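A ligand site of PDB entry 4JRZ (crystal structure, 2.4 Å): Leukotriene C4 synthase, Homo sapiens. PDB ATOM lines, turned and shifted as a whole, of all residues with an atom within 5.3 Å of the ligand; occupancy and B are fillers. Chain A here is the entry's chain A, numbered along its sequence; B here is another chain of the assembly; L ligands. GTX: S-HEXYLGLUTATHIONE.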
ATOM      1  N   ARG A  57     -24.049  -8.141  -5.730  1.00  0.00           N
ATOM      2  CA  ARG A  57     -24.686  -8.651  -6.926  1.00  0.00           C
ATOM      3  C   ARG A  57     -24.049  -9.986  -7.274  1.00  0.00           C
ATOM      4  O   ARG A  57     -24.695 -10.870  -7.852  1.00  0.00           O
ATOM      5  CB  ARG A  57     -24.548  -7.648  -8.060  1.00  0.00           C
ATOM      6  CG  ARG A  57     -25.242  -8.037  -9.339  1.00  0.00           C
ATOM      7  CD  ARG A  57     -26.481  -7.192  -9.567  1.00  0.00           C
ATOM      8  NE  ARG A  57     -27.503  -7.370  -8.532  1.00  0.00           N
ATOM      9  CZ  ARG A  57     -28.457  -8.295  -8.598  1.00  0.00           C
ATOM     10  NH1 ARG A  57     -28.509  -9.104  -9.641  1.00  0.00           N
ATOM     11  NH2 ARG A  57     -29.360  -8.394  -7.621  1.00  0.00           N
ATOM     12  N   ASN A  61     -26.196 -13.412  -7.702  1.00  0.00           N
ATOM     13  CA  ASN A  61     -26.164 -14.203  -8.939  1.00  0.00           C
ATOM     14  C   ASN A  61     -25.823 -15.653  -8.666  1.00  0.00           C
ATOM     15  O   ASN A  61     -26.404 -16.549  -9.257  1.00  0.00           O
ATOM     16  CB  ASN A  61     -25.183 -13.638  -9.972  1.00  0.00           C
ATOM     17  CG  ASN A  61     -25.715 -12.402 -10.705  1.00  0.00           C
ATOM     18  OD1 ASN A  61     -26.922 -12.131 -10.756  1.00  0.00           O
ATOM     19  ND2 ASN A  61     -24.803 -11.650 -11.308  1.00  0.00           N
ATOM     20  N   GLU A  64     -28.784 -17.508  -7.278  1.00  0.00           N
ATOM     21  CA  GLU A  64     -29.840 -17.753  -8.241  1.00  0.00           C
ATOM     22  C   GLU A  64     -29.554 -19.008  -9.058  1.00  0.00           C
ATOM     23  O   GLU A  64     -30.471 -19.691  -9.512  1.00  0.00           O
ATOM     24  CB  GLU A  64     -29.941 -16.592  -9.216  1.00  0.00           C
ATOM     25  CG  GLU A  64     -30.915 -15.545  -8.808  1.00  0.00           C
ATOM     26  CD  GLU A  64     -31.010 -14.404  -9.831  1.00  0.00           C
ATOM     27  OE1 GLU A  64     -30.174 -14.338 -10.775  1.00  0.00           O
ATOM     28  OE2 GLU A  64     -31.933 -13.587  -9.679  1.00  0.00           O
ATOM     29  N   TYR A  65     -28.268 -19.255  -9.292  1.00  0.00           N
ATOM     30  CA  TYR A  65     -27.834 -20.359 -10.106  1.00  0.00           C
ATOM     31  C   TYR A  65     -27.530 -21.633  -9.300  1.00  0.00           C
ATOM     32  O   TYR A  65     -27.427 -22.685  -9.877  1.00  0.00           O
ATOM     33  CB  TYR A  65     -26.605 -19.952 -10.907  1.00  0.00           C
ATOM     34  CG  TYR A  65     -26.977 -19.417 -12.264  1.00  0.00           C
ATOM     35  CD1 TYR A  65     -26.979 -20.247 -13.375  1.00  0.00           C
ATOM     36  CD2 TYR A  65     -27.363 -18.082 -12.424  1.00  0.00           C
ATOM     37  CE1 TYR A  65     -27.341 -19.775 -14.616  1.00  0.00           C
ATOM     38  CE2 TYR A  65     -27.717 -17.593 -13.678  1.00  0.00           C
ATOM     39  CZ  TYR A  65     -27.707 -18.456 -14.761  1.00  0.00           C
ATOM     40  OH  TYR A  65     -28.047 -17.990 -16.004  1.00  0.00           O
ATOM     41  N   ARG A  96     -16.996 -20.470 -10.193  1.00  0.00           N
ATOM     42  CA  ARG A  96     -17.849 -19.575  -9.418  1.00  0.00           C
ATOM     43  C   ARG A  96     -17.096 -18.805  -8.345  1.00  0.00           C
ATOM     44  O   ARG A  96     -17.410 -17.646  -8.076  1.00  0.00           O
ATOM     45  CB  ARG A  96     -19.032 -20.317  -8.810  1.00  0.00           C
ATOM     46  CG  ARG A  96     -20.142 -20.587  -9.794  1.00  0.00           C
ATOM     47  CD  ARG A  96     -20.665 -19.294 -10.348  1.00  0.00           C
ATOM     48  NE  ARG A  96     -21.917 -19.486 -11.072  1.00  0.00           N
ATOM     49  CZ  ARG A  96     -22.614 -18.488 -11.614  1.00  0.00           C
ATOM     50  NH1 ARG A  96     -22.166 -17.241 -11.514  1.00  0.00           N
ATOM     51  NH2 ARG A  96     -23.752 -18.744 -12.260  1.00  0.00           N
ATOM     52  N   TYR A  99     -15.452 -16.133 -10.305  1.00  0.00           N
ATOM     53  CA  TYR A  99     -16.464 -15.157 -10.690  1.00  0.00           C
ATOM     54  C   TYR A  99     -16.667 -14.160  -9.553  1.00  0.00           C
ATOM     55  O   TYR A  99     -16.643 -12.933  -9.742  1.00  0.00           O
ATOM     56  CB  TYR A  99     -17.757 -15.891 -11.081  1.00  0.00           C
ATOM     57  CG  TYR A  99     -18.978 -15.016 -11.289  1.00  0.00           C
ATOM     58  CD1 TYR A  99     -19.289 -14.504 -12.548  1.00  0.00           C
ATOM     59  CD2 TYR A  99     -19.823 -14.723 -10.239  1.00  0.00           C
ATOM     60  CE1 TYR A  99     -20.411 -13.703 -12.732  1.00  0.00           C
ATOM     61  CE2 TYR A  99     -20.946 -13.927 -10.415  1.00  0.00           C
ATOM     62  CZ  TYR A  99     -21.230 -13.419 -11.663  1.00  0.00           C
ATOM     63  OH  TYR A  99     -22.357 -12.632 -11.798  1.00  0.00           O
ATOM     64  N   TYR A 103     -15.546 -10.214  -9.784  1.00  0.00           N
ATOM     65  CA  TYR A 103     -16.619  -9.239  -9.785  1.00  0.00           C
ATOM     66  C   TYR A 103     -16.404  -8.261  -8.632  1.00  0.00           C
ATOM     67  O   TYR A 103     -16.675  -7.074  -8.780  1.00  0.00           O
ATOM     68  CB  TYR A 103     -17.969  -9.946  -9.633  1.00  0.00           C
ATOM     69  CG  TYR A 103     -19.183  -9.191 -10.092  1.00  0.00           C
ATOM     70  CD1 TYR A 103     -19.108  -7.863 -10.520  1.00  0.00           C
ATOM     71  CD2 TYR A 103     -20.431  -9.803 -10.107  1.00  0.00           C
ATOM     72  CE1 TYR A 103     -20.254  -7.174 -10.943  1.00  0.00           C
ATOM     73  CE2 TYR A 103     -21.571  -9.143 -10.524  1.00  0.00           C
ATOM     74  CZ  TYR A 103     -21.483  -7.825 -10.934  1.00  0.00           C
ATOM     75  OH  TYR A 103     -22.636  -7.182 -11.351  1.00  0.00           O
ATOM     76  N   ARG A 110     -15.342 -10.339 -14.019  1.00  0.00           N
ATOM     77  CA  ARG A 110     -16.263 -11.415 -13.702  1.00  0.00           C
ATOM     78  C   ARG A 110     -16.540 -12.250 -14.960  1.00  0.00           C
ATOM     79  O   ARG A 110     -16.976 -13.398 -14.856  1.00  0.00           O
ATOM     80  CB  ARG A 110     -17.573 -10.841 -13.136  1.00  0.00           C
ATOM     81  CG  ARG A 110     -18.698 -10.767 -14.167  1.00  0.00           C
ATOM     82  CD  ARG A 110     -19.865  -9.976 -13.640  1.00  0.00           C
ATOM     83  NE  ARG A 110     -20.937  -9.939 -14.629  1.00  0.00           N
ATOM     84  CZ  ARG A 110     -20.990  -9.111 -15.667  1.00  0.00           C
ATOM     85  NH1 ARG A 110     -22.012  -9.169 -16.510  1.00  0.00           N
ATOM     86  NH2 ARG A 110     -20.007  -8.231 -15.875  1.00  0.00           N
ATOM     87  N   LEU A 114     -17.185 -16.303 -15.532  1.00  0.00           N
ATOM     88  CA  LEU A 114     -18.584 -16.559 -15.860  1.00  0.00           C
ATOM     89  C   LEU A 114     -18.718 -17.517 -17.051  1.00  0.00           C
ATOM     90  O   LEU A 114     -19.565 -18.403 -17.058  1.00  0.00           O
ATOM     91  CB  LEU A 114     -19.363 -15.280 -16.128  1.00  0.00           C
ATOM     92  CG  LEU A 114     -20.828 -15.511 -16.505  1.00  0.00           C
ATOM     93  CD1 LEU A 114     -21.586 -16.164 -15.341  1.00  0.00           C
ATOM     94  CD2 LEU A 114     -21.524 -14.248 -16.965  1.00  0.00           C
ATOM     95  N   ALA A 118     -20.452 -21.202 -17.035  1.00  0.00           N
ATOM     96  CA  ALA A 118     -21.583 -21.568 -17.879  1.00  0.00           C
ATOM     97  C   ALA A 118     -21.280 -22.771 -18.792  1.00  0.00           C
ATOM     98  O   ALA A 118     -22.178 -23.528 -19.149  1.00  0.00           O
ATOM     99  CB  ALA A 118     -22.069 -20.400 -18.697  1.00  0.00           C
ATOM    100  N   LEU A 121     -21.740 -25.746 -16.542  1.00  0.00           N
ATOM    101  CA  LEU A 121     -23.170 -25.940 -16.302  1.00  0.00           C
ATOM    102  C   LEU A 121     -23.833 -26.521 -17.520  1.00  0.00           C
ATOM    103  O   LEU A 121     -24.749 -27.349 -17.415  1.00  0.00           O
ATOM    104  CB  LEU A 121     -23.854 -24.632 -15.915  1.00  0.00           C
ATOM    105  CG  LEU A 121     -25.316 -24.781 -15.508  1.00  0.00           C
ATOM    106  CD1 LEU A 121     -25.470 -25.795 -14.358  1.00  0.00           C
ATOM    107  CD2 LEU A 121     -25.911 -23.442 -15.094  1.00  0.00           C
ATOM    108  N   PHE A 122     -23.348 -26.095 -18.687  1.00  0.00           N
ATOM    109  CA  PHE A 122     -23.857 -26.592 -19.957  1.00  0.00           C
ATOM    110  C   PHE A 122     -23.527 -28.063 -20.136  1.00  0.00           C
ATOM    111  O   PHE A 122     -24.304 -28.837 -20.693  1.00  0.00           O
ATOM    112  CB  PHE A 122     -23.250 -25.807 -21.124  1.00  0.00           C
ATOM    113  CG  PHE A 122     -23.615 -26.388 -22.468  1.00  0.00           C
ATOM    114  CD1 PHE A 122     -24.824 -26.068 -23.057  1.00  0.00           C
ATOM    115  CD2 PHE A 122     -22.753 -27.265 -23.124  1.00  0.00           C
ATOM    116  CE1 PHE A 122     -25.180 -26.613 -24.283  1.00  0.00           C
ATOM    117  CE2 PHE A 122     -23.095 -27.809 -24.349  1.00  0.00           C
ATOM    118  CZ  PHE A 122     -24.305 -27.477 -24.930  1.00  0.00           C
ATOM    119  N   VAL A 125     -25.882 -30.183 -18.040  1.00  0.00           N
ATOM    120  CA  VAL A 125     -27.214 -30.258 -18.626  1.00  0.00           C
ATOM    121  C   VAL A 125     -27.208 -31.258 -19.783  1.00  0.00           C
ATOM    122  O   VAL A 125     -28.204 -31.957 -20.031  1.00  0.00           O
ATOM    123  CB  VAL A 125     -27.685 -28.852 -19.140  1.00  0.00           C
ATOM    124  CG1 VAL A 125     -28.982 -28.950 -19.928  1.00  0.00           C
ATOM    125  CG2 VAL A 125     -27.826 -27.858 -17.976  1.00  0.00           C
ATOM    126  N   ALA B  26     -32.830 -21.149 -17.520  1.00  0.00           N
ATOM    127  CA  ALA B  26     -31.700 -20.670 -18.274  1.00  0.00           C
ATOM    128  C   ALA B  26     -32.228 -19.805 -19.403  1.00  0.00           C
ATOM    129  O   ALA B  26     -31.620 -18.810 -19.777  1.00  0.00           O
ATOM    130  CB  ALA B  26     -30.861 -21.829 -18.800  1.00  0.00           C
ATOM    131  N   PHE B  28     -34.907 -18.007 -19.172  1.00  0.00           N
ATOM    132  CA  PHE B  28     -35.276 -16.751 -18.528  1.00  0.00           C
ATOM    133  C   PHE B  28     -34.032 -15.899 -18.362  1.00  0.00           C
ATOM    134  O   PHE B  28     -34.073 -14.690 -18.545  1.00  0.00           O
ATOM    135  CB  PHE B  28     -35.882 -17.027 -17.160  1.00  0.00           C
ATOM    136  CG  PHE B  28     -37.239 -17.614 -17.230  1.00  0.00           C
ATOM    137  CD1 PHE B  28     -37.940 -17.628 -18.428  1.00  0.00           C
ATOM    138  CD2 PHE B  28     -37.831 -18.188 -16.106  1.00  0.00           C
ATOM    139  CE1 PHE B  28     -39.212 -18.180 -18.491  1.00  0.00           C
ATOM    140  CE2 PHE B  28     -39.089 -18.739 -16.168  1.00  0.00           C
ATOM    141  CZ  PHE B  28     -39.783 -18.730 -17.363  1.00  0.00           C
ATOM    142  N   SER B  29     -32.935 -16.558 -18.020  1.00  0.00           N
ATOM    143  CA  SER B  29     -31.656 -15.872 -17.837  1.00  0.00           C
ATOM    144  C   SER B  29     -31.132 -15.246 -19.135  1.00  0.00           C
ATOM    145  O   SER B  29     -30.546 -14.175 -19.109  1.00  0.00           O
ATOM    146  CB  SER B  29     -30.621 -16.830 -17.262  1.00  0.00           C
ATOM    147  OG  SER B  29     -30.918 -17.140 -15.921  1.00  0.00           O
ATOM    148  N   LEU B  30     -31.342 -15.933 -20.247  1.00  0.00           N
ATOM    149  CA  LEU B  30     -30.910 -15.428 -21.535  1.00  0.00           C
ATOM    150  C   LEU B  30     -31.731 -14.198 -21.944  1.00  0.00           C
ATOM    151  O   LEU B  30     -31.187 -13.263 -22.527  1.00  0.00           O
ATOM    152  CB  LEU B  30     -30.975 -16.523 -22.616  1.00  0.00           C
ATOM    153  CG  LEU B  30     -29.883 -17.590 -22.518  1.00  0.00           C
ATOM    154  CD1 LEU B  30     -30.063 -18.668 -23.587  1.00  0.00           C
ATOM    155  CD2 LEU B  30     -28.500 -16.961 -22.633  1.00  0.00           C
ATOM    156  N   VAL B  32     -33.060 -11.987 -19.907  1.00  0.00           N
ATOM    157  CA  VAL B  32     -32.648 -10.854 -19.100  1.00  0.00           C
ATOM    158  C   VAL B  32     -31.342 -10.262 -19.636  1.00  0.00           C
ATOM    159  O   VAL B  32     -31.160  -9.047 -19.640  1.00  0.00           O
ATOM    160  CB  VAL B  32     -32.498 -11.232 -17.607  1.00  0.00           C
ATOM    161  CG1 VAL B  32     -31.774 -10.134 -16.852  1.00  0.00           C
ATOM    162  CG2 VAL B  32     -33.873 -11.455 -17.001  1.00  0.00           C
ATOM    163  N   ILE B  33     -30.448 -11.117 -20.122  1.00  0.00           N
ATOM    164  CA  ILE B  33     -29.243 -10.644 -20.777  1.00  0.00           C
ATOM    165  C   ILE B  33     -29.596  -9.897 -22.071  1.00  0.00           C
ATOM    166  O   ILE B  33     -28.945  -8.931 -22.446  1.00  0.00           O
ATOM    167  CB  ILE B  33     -28.271 -11.800 -21.076  1.00  0.00           C
ATOM    168  CG1 ILE B  33     -27.808 -12.417 -19.762  1.00  0.00           C
ATOM    169  CG2 ILE B  33     -27.084 -11.313 -21.902  1.00  0.00           C
ATOM    170  CD1 ILE B  33     -26.371 -12.830 -19.790  1.00  0.00           C
ATOM    171  N   ARG B  36     -31.063  -6.518 -20.984  1.00  0.00           N
ATOM    172  CA  ARG B  36     -29.935  -5.687 -20.595  1.00  0.00           C
ATOM    173  C   ARG B  36     -29.256  -5.038 -21.817  1.00  0.00           C
ATOM    174  O   ARG B  36     -28.824  -3.892 -21.757  1.00  0.00           O
ATOM    175  CB  ARG B  36     -28.895  -6.489 -19.814  1.00  0.00           C
ATOM    176  CG  ARG B  36     -29.175  -6.645 -18.329  1.00  0.00           C
ATOM    177  CD  ARG B  36     -27.941  -7.153 -17.608  1.00  0.00           C
ATOM    178  NE  ARG B  36     -28.195  -7.488 -16.208  1.00  0.00           N
ATOM    179  CZ  ARG B  36     -28.182  -6.606 -15.206  1.00  0.00           C
ATOM    180  NH1 ARG B  36     -27.962  -5.323 -15.448  1.00  0.00           N
ATOM    181  NH2 ARG B  36     -28.404  -7.025 -13.963  1.00  0.00           N
ATOM    182  N   THR B  46     -29.846  -2.972 -11.293  1.00  0.00           N
ATOM    183  CA  THR B  46     -30.981  -3.774 -11.689  1.00  0.00           C
ATOM    184  C   THR B  46     -32.198  -2.891 -11.938  1.00  0.00           C
ATOM    185  O   THR B  46     -33.340  -3.364 -11.963  1.00  0.00           O
ATOM    186  CB  THR B  46     -31.263  -4.834 -10.603  1.00  0.00           C
ATOM    187  OG1 THR B  46     -31.605  -4.178  -9.374  1.00  0.00           O
ATOM    188  CG2 THR B  46     -30.011  -5.671 -10.358  1.00  0.00           C
ATOM    189  N   TYR B  56     -36.597  -8.401 -15.680  1.00  0.00           N
ATOM    190  CA  TYR B  56     -35.680  -8.711 -14.604  1.00  0.00           C
ATOM    191  C   TYR B  56     -36.425  -9.245 -13.376  1.00  0.00           C
ATOM    192  O   TYR B  56     -35.943 -10.149 -12.688  1.00  0.00           O
ATOM    193  CB  TYR B  56     -34.854  -7.496 -14.228  1.00  0.00           C
ATOM    194  CG  TYR B  56     -34.051  -7.675 -12.962  1.00  0.00           C
ATOM    195  CD1 TYR B  56     -32.801  -8.286 -13.002  1.00  0.00           C
ATOM    196  CD2 TYR B  56     -34.539  -7.235 -11.740  1.00  0.00           C
ATOM    197  CE1 TYR B  56     -32.073  -8.471 -11.842  1.00  0.00           C
ATOM    198  CE2 TYR B  56     -33.817  -7.409 -10.585  1.00  0.00           C
ATOM    199  CZ  TYR B  56     -32.579  -8.027 -10.642  1.00  0.00           C
ATOM    200  OH  TYR B  56     -31.828  -8.196  -9.493  1.00  0.00           O
ATOM    201  N   GLN B  59     -37.707 -12.934 -13.957  1.00  0.00           N
ATOM    202  CA  GLN B  59     -36.650 -13.907 -13.732  1.00  0.00           C
ATOM    203  C   GLN B  59     -36.395 -14.116 -12.242  1.00  0.00           C
ATOM    204  O   GLN B  59     -36.393 -15.268 -11.767  1.00  0.00           O
ATOM    205  CB  GLN B  59     -35.376 -13.447 -14.424  1.00  0.00           C
ATOM    206  CG  GLN B  59     -34.168 -14.351 -14.225  1.00  0.00           C
ATOM    207  CD  GLN B  59     -33.265 -13.861 -13.124  1.00  0.00           C
ATOM    208  OE1 GLN B  59     -32.734 -12.750 -13.183  1.00  0.00           O
ATOM    209  NE2 GLN B  59     -33.082 -14.672 -12.099  1.00  0.00           N
HETATM  210  N1  GTX L   1     -29.913 -12.063 -12.511  1.00  0.00           N
HETATM  211  CA1 GTX L   1     -29.298 -11.899 -13.805  1.00  0.00           C
HETATM  212  C1  GTX L   1     -29.043 -10.443 -14.066  1.00  0.00           C
HETATM  213  O11 GTX L   1     -28.261 -10.094 -15.004  1.00  0.00           O
HETATM  214  O12 GTX L   1     -29.612  -9.561 -13.355  1.00  0.00           O
HETATM  215  CB1 GTX L   1     -30.248 -12.491 -14.786  1.00  0.00           C
HETATM  216  CG1 GTX L   1     -29.760 -13.095 -16.052  1.00  0.00           C
HETATM  217  CD1 GTX L   1     -28.627 -14.025 -15.887  1.00  0.00           C
HETATM  218  OE1 GTX L   1     -28.505 -14.650 -14.847  1.00  0.00           O
HETATM  219  N2  GTX L   1     -27.657 -14.218 -16.922  1.00  0.00           N
HETATM  220  CA2 GTX L   1     -26.601 -15.129 -16.623  1.00  0.00           C
HETATM  221  C2  GTX L   1     -25.650 -14.381 -15.746  1.00  0.00           C
HETATM  222  O2  GTX L   1     -24.583 -14.873 -15.408  1.00  0.00           O
HETATM  223  CB2 GTX L   1     -25.925 -15.621 -17.872  1.00  0.00           C
HETATM  224  SG2 GTX L   1     -26.918 -16.286 -19.186  1.00  0.00           S
HETATM  225  C1S GTX L   1     -26.634 -18.025 -19.288  1.00  0.00           C
HETATM  226  C2S GTX L   1     -27.772 -18.943 -19.023  1.00  0.00           C
HETATM  227  C3S GTX L   1     -27.468 -20.270 -18.416  1.00  0.00           C
HETATM  228  C4S GTX L   1     -26.440 -21.112 -19.094  1.00  0.00           C
HETATM  229  C5S GTX L   1     -26.825 -22.488 -19.517  1.00  0.00           C
HETATM  230  C6S GTX L   1     -25.696 -23.419 -19.863  1.00  0.00           C
HETATM  231  N3  GTX L   1     -26.041 -13.068 -15.305  1.00  0.00           N
HETATM  232  CA3 GTX L   1     -25.195 -12.287 -14.453  1.00  0.00           C
HETATM  233  C3  GTX L   1     -23.881 -11.935 -15.032  1.00  0.00           C
HETATM  234  O31 GTX L   1     -22.888 -11.801 -14.274  1.00  0.00           O
HETATM  235  O32 GTX L   1     -23.804 -11.796 -16.286  1.00  0.00           O
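Leu 114 touches the ligand. O of Ala 118 touches C6S of the ligand, at 3.6 Å. CB of Phe 122 touches C6S of the ligand, at 3.6 Å. CB of Ala 26 of chain B touches C3S of the ligand, 3.8 Å away. Ser 29 of chain B touches the ligand. CD2 of Leu 30 of chain B touches SG2 of the ligand (3.9 Å). Val 32 of chain B touches the ligand (CG1 to CB1, 3.5 Å). Ile 33 of chain B touches the ligand (CG1 to N2, 3.4 Å). Tyr 56 of chain B touches the ligand. Hydrophobic or aromatic side chains that line the ligand: Tyr 65, Tyr 99, Leu 114, Phe 122, Ala 26 of chain B, Leu 30 of chain B, Val 32 of chain B, Ile 33 of chain B and Tyr 56 of chain B. Within 4 Å of the ligand: Arg 57, Asn 61, Glu 64, Tyr 65, Tyr 99, Arg 110, Leu 114, Ala 118, Phe 122, Ala 26 of chain B, Ser 29 of chain B, Leu 30 of chain B, Val 32 of chain B, Ile 33 of chain B, Arg 36 of chain B, Tyr 56 of chain B and Gln 59 of chain B.
The side-chain hydroxyl (OH) of Tyr 99 lies within hydrogen-bond range of the side-chain amide nitrogen (ND2) of Asn 61. The side-chain carboxylate of Glu 64 lies within hydrogen-bond range of the side-chain amide nitrogen of Gln 59 of chain B (2.9 Å). The side-chain hydroxyl (OH) of Tyr 56 of chain B lies within hydrogen-bond range of the guanidinium group (NH2) of Arg 57, at 3.1 Å. The side-chain hydroxyl of Tyr 65 is in hydrogen-bond range of the side-chain hydroxyl of Ser 29 of chain B, 3.0 Å away.
OH of Tyr 99 sits at hydrogen-bond distance from O31 of the ligand. The guanidinium group of Arg 110 is in salt-bridge range of an oxygen (O31) of the ligand (2.7 Å). The guanidinium group (NE) of Arg 36 of chain B is in salt-bridge range of an oxygen (O11) of the ligand (2.9 Å). OE1 of Glu 64 is in salt-bridge range of N1 of the ligand. OE1 of Gln 59 of chain B sits close to N1 of the ligand (3.0 Å). The side-chain hydroxyl of Tyr 65 sits close to a sulfur (SG2) of the ligand. The side-chain amide oxygen of Asn 61 lies within hydrogen-bond range of a nitrogen (N1) of the ligand, at 3.5 Å. The guanidinium group (NH1) of Arg 57 is in salt-bridge range of an oxygen (O12) of the ligand, 3.9 Å away.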
